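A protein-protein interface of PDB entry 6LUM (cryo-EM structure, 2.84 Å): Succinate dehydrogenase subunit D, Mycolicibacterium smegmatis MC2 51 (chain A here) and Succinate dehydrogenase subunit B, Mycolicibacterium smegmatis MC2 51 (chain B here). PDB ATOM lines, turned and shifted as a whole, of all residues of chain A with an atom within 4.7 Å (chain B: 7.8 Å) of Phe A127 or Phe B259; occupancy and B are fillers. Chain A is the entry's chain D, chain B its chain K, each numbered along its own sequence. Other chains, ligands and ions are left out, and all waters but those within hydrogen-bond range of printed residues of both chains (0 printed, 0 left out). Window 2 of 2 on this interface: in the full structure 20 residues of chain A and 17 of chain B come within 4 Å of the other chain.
The guanidinium group of Arg B255 lies within salt-bridge range of the side-chain carboxylate of Asp A23 (3.0 Å).
OG of Ser A131 is in hydrogen-bond range of O of Phe A127, at 3.0 Å.
Among the printed residues, merely in contact across the chains: Asp A23 with Ala B256 (3.7 Å), Asp A23 with Phe B259 (3.3 Å), Asn A123 with Phe B259 (3.3 Å), Val A124 with Phe B259 (3.8 Å) and Phe A127 with Phe B259 (3.5 Å).
Of the printed residues of chain B, Asp A23 touches Arg B255 (3.0 Å), Ala B256 (3.7 Å) and Phe B259 (3.3 Å).
Of the printed residues of chain B, Val A124 touches Phe B259 (3.8 Å).
Val B253 touches none of the printed residues of chain A.
Of the printed residues of chain A, Arg B255 touches Asp A23 (3.0 Å).
Printed residues of chain A within 4 Å of Ala B256: Asp A23 (3.7 Å).
Met B258 touches none of the printed residues of chain A.
Of chain A, only Asp A23 (3.3 Å), Asn A123 (3.3 Å), Val A124 (3.8 Å) and Phe A127 (3.5 Å) come within 4 Å of Phe B259.
The nearest printed residue of chain B that does not touch Asn A123 is Ala B260 (4.7 Å).
Along chain A the printed residues that touch a printed residue of chain B span positions 23 to 127.
Hydrophobic or aromatic side chains of chain B within 4 Å of the printed part of chain A: Ala B256 and Phe B259.
Along chain B the printed residues that touch a printed residue of chain A span positions 255 to 259.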
ATOM      1  N   ASP A  23      -1.985 -16.464 -31.153  1.00  0.00           N
ATOM      2  CA  ASP A  23      -1.124 -17.198 -30.239  1.00  0.00           C
ATOM      3  C   ASP A  23       0.355 -16.964 -30.497  1.00  0.00           C
ATOM      4  O   ASP A  23       1.186 -17.522 -29.778  1.00  0.00           O
ATOM      5  CB  ASP A  23      -1.430 -18.689 -30.347  1.00  0.00           C
ATOM      6  CG  ASP A  23      -2.841 -19.014 -29.939  1.00  0.00           C
ATOM      7  OD1 ASP A  23      -3.377 -18.319 -29.056  1.00  0.00           O
ATOM      8  OD2 ASP A  23      -3.429 -19.948 -30.515  1.00  0.00           O
ATOM      9  N   ASN A 123       0.623 -22.405 -36.425  1.00  0.00           N
ATOM     10  CA  ASN A 123       1.162 -23.232 -35.357  1.00  0.00           C
ATOM     11  C   ASN A 123       0.080 -24.057 -34.684  1.00  0.00           C
ATOM     12  O   ASN A 123       0.366 -25.136 -34.162  1.00  0.00           O
ATOM     13  CB  ASN A 123       1.870 -22.359 -34.336  1.00  0.00           C
ATOM     14  CG  ASN A 123       2.967 -21.544 -34.947  1.00  0.00           C
ATOM     15  OD1 ASN A 123       2.756 -20.403 -35.333  1.00  0.00           O
ATOM     16  ND2 ASN A 123       4.150 -22.123 -35.045  1.00  0.00           N
ATOM     17  N   VAL A 124      -1.164 -23.592 -34.712  1.00  0.00           N
ATOM     18  CA  VAL A 124      -2.255 -24.391 -34.173  1.00  0.00           C
ATOM     19  C   VAL A 124      -2.515 -25.598 -35.058  1.00  0.00           C
ATOM     20  O   VAL A 124      -2.716 -26.715 -34.568  1.00  0.00           O
ATOM     21  CB  VAL A 124      -3.510 -23.523 -34.015  1.00  0.00           C
ATOM     22  CG1 VAL A 124      -4.572 -24.278 -33.283  1.00  0.00           C
ATOM     23  CG2 VAL A 124      -3.172 -22.262 -33.284  1.00  0.00           C
ATOM     24  N   THR A 125      -2.521 -25.398 -36.375  1.00  0.00           N
ATOM     25  CA  THR A 125      -2.661 -26.520 -37.293  1.00  0.00           C
ATOM     26  C   THR A 125      -1.526 -27.507 -37.120  1.00  0.00           C
ATOM     27  O   THR A 125      -1.743 -28.719 -37.123  1.00  0.00           O
ATOM     28  CB  THR A 125      -2.699 -26.026 -38.731  1.00  0.00           C
ATOM     29  OG1 THR A 125      -3.637 -24.955 -38.841  1.00  0.00           O
ATOM     30  CG2 THR A 125      -3.122 -27.134 -39.641  1.00  0.00           C
ATOM     31  N   LYS A 126      -0.304 -27.006 -36.975  1.00  0.00           N
ATOM     32  CA  LYS A 126       0.829 -27.889 -36.761  1.00  0.00           C
ATOM     33  C   LYS A 126       0.666 -28.697 -35.482  1.00  0.00           C
ATOM     34  O   LYS A 126       0.905 -29.907 -35.472  1.00  0.00           O
ATOM     35  CB  LYS A 126       2.106 -27.067 -36.727  1.00  0.00           C
ATOM     36  CG  LYS A 126       3.354 -27.844 -36.921  1.00  0.00           C
ATOM     37  CD  LYS A 126       4.540 -26.971 -36.667  1.00  0.00           C
ATOM     38  CE  LYS A 126       5.734 -27.799 -36.304  1.00  0.00           C
ATOM     39  NZ  LYS A 126       6.807 -26.972 -35.717  1.00  0.00           N
ATOM     40  N   PHE A 127       0.241 -28.050 -34.397  1.00  0.00           N
ATOM     41  CA  PHE A 127       0.052 -28.751 -33.132  1.00  0.00           C
ATOM     42  C   PHE A 127      -0.981 -29.859 -33.260  1.00  0.00           C
ATOM     43  O   PHE A 127      -0.747 -30.996 -32.839  1.00  0.00           O
ATOM     44  CB  PHE A 127      -0.363 -27.757 -32.051  1.00  0.00           C
ATOM     45  CG  PHE A 127      -0.557 -28.375 -30.703  1.00  0.00           C
ATOM     46  CD1 PHE A 127       0.516 -28.595 -29.871  1.00  0.00           C
ATOM     47  CD2 PHE A 127      -1.809 -28.733 -30.265  1.00  0.00           C
ATOM     48  CE1 PHE A 127       0.338 -29.163 -28.648  1.00  0.00           C
ATOM     49  CE2 PHE A 127      -1.983 -29.300 -29.040  1.00  0.00           C
ATOM     50  CZ  PHE A 127      -0.913 -29.512 -28.234  1.00  0.00           C
ATOM     51  N   TRP A 128      -2.133 -29.553 -33.844  1.00  0.00           N
ATOM     52  CA  TRP A 128      -3.196 -30.545 -33.879  1.00  0.00           C
ATOM     53  C   TRP A 128      -2.932 -31.643 -34.896  1.00  0.00           C
ATOM     54  O   TRP A 128      -3.354 -32.783 -34.686  1.00  0.00           O
ATOM     55  CB  TRP A 128      -4.532 -29.867 -34.145  1.00  0.00           C
ATOM     56  CG  TRP A 128      -5.007 -29.096 -32.964  1.00  0.00           C
ATOM     57  CD1 TRP A 128      -5.203 -27.757 -32.893  1.00  0.00           C
ATOM     58  CD2 TRP A 128      -5.326 -29.616 -31.674  1.00  0.00           C
ATOM     59  NE1 TRP A 128      -5.633 -27.408 -31.643  1.00  0.00           N
ATOM     60  CE2 TRP A 128      -5.715 -28.535 -30.875  1.00  0.00           C
ATOM     61  CE3 TRP A 128      -5.325 -30.895 -31.117  1.00  0.00           C
ATOM     62  CZ2 TRP A 128      -6.098 -28.691 -29.555  1.00  0.00           C
ATOM     63  CZ3 TRP A 128      -5.703 -31.045 -29.811  1.00  0.00           C
ATOM     64  CH2 TRP A 128      -6.085 -29.953 -29.043  1.00  0.00           C
ATOM     65  N   LEU A 129      -2.200 -31.355 -35.969  1.00  0.00           N
ATOM     66  CA  LEU A 129      -1.842 -32.417 -36.899  1.00  0.00           C
ATOM     67  C   LEU A 129      -0.768 -33.320 -36.320  1.00  0.00           C
ATOM     68  O   LEU A 129      -0.792 -34.529 -36.546  1.00  0.00           O
ATOM     69  CB  LEU A 129      -1.385 -31.826 -38.223  1.00  0.00           C
ATOM     70  CG  LEU A 129      -2.451 -31.330 -39.185  1.00  0.00           C
ATOM     71  CD1 LEU A 129      -1.778 -30.758 -40.383  1.00  0.00           C
ATOM     72  CD2 LEU A 129      -3.355 -32.443 -39.588  1.00  0.00           C
ATOM     73  N   ASN A 130       0.179 -32.767 -35.567  1.00  0.00           N
ATOM     74  CA  ASN A 130       1.136 -33.621 -34.876  1.00  0.00           C
ATOM     75  C   ASN A 130       0.460 -34.477 -33.820  1.00  0.00           C
ATOM     76  O   ASN A 130       0.869 -35.617 -33.598  1.00  0.00           O
ATOM     77  CB  ASN A 130       2.234 -32.783 -34.234  1.00  0.00           C
ATOM     78  CG  ASN A 130       3.294 -32.356 -35.213  1.00  0.00           C
ATOM     79  OD1 ASN A 130       3.658 -33.094 -36.114  1.00  0.00           O
ATOM     80  ND2 ASN A 130       3.807 -31.157 -35.033  1.00  0.00           N
ATOM     81  N   SER A 131      -0.576 -33.958 -33.163  1.00  0.00           N
ATOM     82  CA  SER A 131      -1.311 -34.767 -32.196  1.00  0.00           C
ATOM     83  C   SER A 131      -2.082 -35.891 -32.871  1.00  0.00           C
ATOM     84  O   SER A 131      -2.079 -37.026 -32.389  1.00  0.00           O
ATOM     85  CB  SER A 131      -2.256 -33.884 -31.396  1.00  0.00           C
ATOM     86  OG  SER A 131      -1.524 -32.929 -30.662  1.00  0.00           O
ATOM     87  N   TRP B 228       3.975 -23.399 -15.724  1.00  0.00           N
ATOM     88  CA  TRP B 228       3.344 -24.709 -15.665  1.00  0.00           C
ATOM     89  C   TRP B 228       2.934 -25.109 -14.263  1.00  0.00           C
ATOM     90  O   TRP B 228       2.363 -26.185 -14.092  1.00  0.00           O
ATOM     91  CB  TRP B 228       4.276 -25.781 -16.230  1.00  0.00           C
ATOM     92  CG  TRP B 228       4.817 -25.475 -17.570  1.00  0.00           C
ATOM     93  CD1 TRP B 228       6.112 -25.289 -17.889  1.00  0.00           C
ATOM     94  CD2 TRP B 228       4.081 -25.325 -18.779  1.00  0.00           C
ATOM     95  NE1 TRP B 228       6.238 -25.022 -19.218  1.00  0.00           N
ATOM     96  CE2 TRP B 228       4.996 -25.039 -19.787  1.00  0.00           C
ATOM     97  CE3 TRP B 228       2.732 -25.394 -19.104  1.00  0.00           C
ATOM     98  CZ2 TRP B 228       4.611 -24.832 -21.092  1.00  0.00           C
ATOM     99  CZ3 TRP B 228       2.359 -25.187 -20.393  1.00  0.00           C
ATOM    100  CH2 TRP B 228       3.284 -24.912 -21.372  1.00  0.00           C
ATOM    101  N   GLU B 252      -2.703 -17.318 -22.009  1.00  0.00           N
ATOM    102  CA  GLU B 252      -2.114 -16.905 -23.274  1.00  0.00           C
ATOM    103  C   GLU B 252      -0.623 -17.173 -23.308  1.00  0.00           C
ATOM    104  O   GLU B 252      -0.087 -17.530 -24.357  1.00  0.00           O
ATOM    105  CB  GLU B 252      -2.387 -15.436 -23.527  1.00  0.00           C
ATOM    106  CG  GLU B 252      -3.842 -15.123 -23.675  1.00  0.00           C
ATOM    107  CD  GLU B 252      -4.077 -13.717 -24.155  1.00  0.00           C
ATOM    108  OE1 GLU B 252      -3.148 -13.132 -24.742  1.00  0.00           O
ATOM    109  OE2 GLU B 252      -5.188 -13.190 -23.951  1.00  0.00           O
ATOM    110  N   VAL B 253       0.064 -17.029 -22.179  1.00  0.00           N
ATOM    111  CA  VAL B 253       1.479 -17.395 -22.165  1.00  0.00           C
ATOM    112  C   VAL B 253       1.649 -18.904 -22.323  1.00  0.00           C
ATOM    113  O   VAL B 253       2.549 -19.374 -23.028  1.00  0.00           O
ATOM    114  CB  VAL B 253       2.157 -16.879 -20.890  1.00  0.00           C
ATOM    115  CG1 VAL B 253       3.577 -17.346 -20.844  1.00  0.00           C
ATOM    116  CG2 VAL B 253       2.107 -15.380 -20.849  1.00  0.00           C
ATOM    117  N   LYS B 254       0.780 -19.689 -21.687  1.00  0.00           N
ATOM    118  CA  LYS B 254       0.838 -21.139 -21.855  1.00  0.00           C
ATOM    119  C   LYS B 254       0.628 -21.539 -23.304  1.00  0.00           C
ATOM    120  O   LYS B 254       1.317 -22.420 -23.819  1.00  0.00           O
ATOM    121  CB  LYS B 254      -0.215 -21.812 -20.987  1.00  0.00           C
ATOM    122  CG  LYS B 254       0.242 -22.194 -19.619  1.00  0.00           C
ATOM    123  CD  LYS B 254      -0.953 -22.380 -18.746  1.00  0.00           C
ATOM    124  CE  LYS B 254      -0.586 -22.957 -17.425  1.00  0.00           C
ATOM    125  NZ  LYS B 254      -1.809 -23.162 -16.638  1.00  0.00           N
ATOM    126  N   ARG B 255      -0.334 -20.919 -23.976  1.00  0.00           N
ATOM    127  CA  ARG B 255      -0.611 -21.279 -25.358  1.00  0.00           C
ATOM    128  C   ARG B 255       0.474 -20.784 -26.296  1.00  0.00           C
ATOM    129  O   ARG B 255       0.745 -21.423 -27.311  1.00  0.00           O
ATOM    130  CB  ARG B 255      -1.967 -20.744 -25.773  1.00  0.00           C
ATOM    131  CG  ARG B 255      -3.091 -21.552 -25.212  1.00  0.00           C
ATOM    132  CD  ARG B 255      -4.375 -20.807 -25.268  1.00  0.00           C
ATOM    133  NE  ARG B 255      -4.704 -20.419 -26.624  1.00  0.00           N
ATOM    134  CZ  ARG B 255      -5.388 -21.180 -27.462  1.00  0.00           C
ATOM    135  NH1 ARG B 255      -5.808 -22.367 -27.080  1.00  0.00           N
ATOM    136  NH2 ARG B 255      -5.648 -20.753 -28.684  1.00  0.00           N
ATOM    137  N   ALA B 256       1.114 -19.661 -25.978  1.00  0.00           N
ATOM    138  CA  ALA B 256       2.279 -19.239 -26.736  1.00  0.00           C
ATOM    139  C   ALA B 256       3.453 -20.177 -26.552  1.00  0.00           C
ATOM    140  O   ALA B 256       4.328 -20.224 -27.413  1.00  0.00           O
ATOM    141  CB  ALA B 256       2.690 -17.831 -26.329  1.00  0.00           C
ATOM    142  N   LEU B 257       3.515 -20.896 -25.437  1.00  0.00           N
ATOM    143  CA  LEU B 257       4.554 -21.909 -25.283  1.00  0.00           C
ATOM    144  C   LEU B 257       4.174 -23.232 -25.937  1.00  0.00           C
ATOM    145  O   LEU B 257       5.056 -23.968 -26.383  1.00  0.00           O
ATOM    146  CB  LEU B 257       4.862 -22.133 -23.808  1.00  0.00           C
ATOM    147  CG  LEU B 257       5.803 -21.141 -23.145  1.00  0.00           C
ATOM    148  CD1 LEU B 257       5.787 -21.337 -21.665  1.00  0.00           C
ATOM    149  CD2 LEU B 257       7.187 -21.334 -23.669  1.00  0.00           C
ATOM    150  N   MET B 258       2.883 -23.558 -25.988  1.00  0.00           N
ATOM    151  CA  MET B 258       2.443 -24.770 -26.674  1.00  0.00           C
ATOM    152  C   MET B 258       2.616 -24.644 -28.179  1.00  0.00           C
ATOM    153  O   MET B 258       3.245 -25.493 -28.815  1.00  0.00           O
ATOM    154  CB  MET B 258       0.982 -25.068 -26.363  1.00  0.00           C
ATOM    155  CG  MET B 258       0.718 -25.769 -25.070  1.00  0.00           C
ATOM    156  SD  MET B 258      -0.928 -25.352 -24.477  1.00  0.00           S
ATOM    157  CE  MET B 258      -1.913 -25.790 -25.894  1.00  0.00           C
ATOM    158  N   PHE B 259       2.042 -23.601 -28.769  1.00  0.00           N
ATOM    159  CA  PHE B 259       2.069 -23.399 -30.214  1.00  0.00           C
ATOM    160  C   PHE B 259       3.245 -22.539 -30.650  1.00  0.00           C
ATOM    161  O   PHE B 259       3.061 -21.587 -31.398  1.00  0.00           O
ATOM    162  CB  PHE B 259       0.766 -22.762 -30.670  1.00  0.00           C
ATOM    163  CG  PHE B 259      -0.462 -23.392 -30.110  1.00  0.00           C
ATOM    164  CD1 PHE B 259      -0.537 -24.737 -29.893  1.00  0.00           C
ATOM    165  CD2 PHE B 259      -1.564 -22.627 -29.832  1.00  0.00           C
ATOM    166  CE1 PHE B 259      -1.675 -25.295 -29.392  1.00  0.00           C
ATOM    167  CE2 PHE B 259      -2.695 -23.189 -29.334  1.00  0.00           C
ATOM    168  CZ  PHE B 259      -2.751 -24.522 -29.115  1.00  0.00           C
ATOM    169  N   ALA B 260       4.453 -22.870 -30.207  1.00  0.00           N
ATOM    170  CA  ALA B 260       5.669 -22.146 -30.585  1.00  0.00           C
ATOM    171  C   ALA B 260       6.876 -22.737 -29.877  1.00  0.00           C
ATOM    172  O   ALA B 260       7.576 -22.039 -29.144  1.00  0.00           O
ATOM    173  CB  ALA B 260       5.562 -20.671 -30.264  1.00  0.00           C
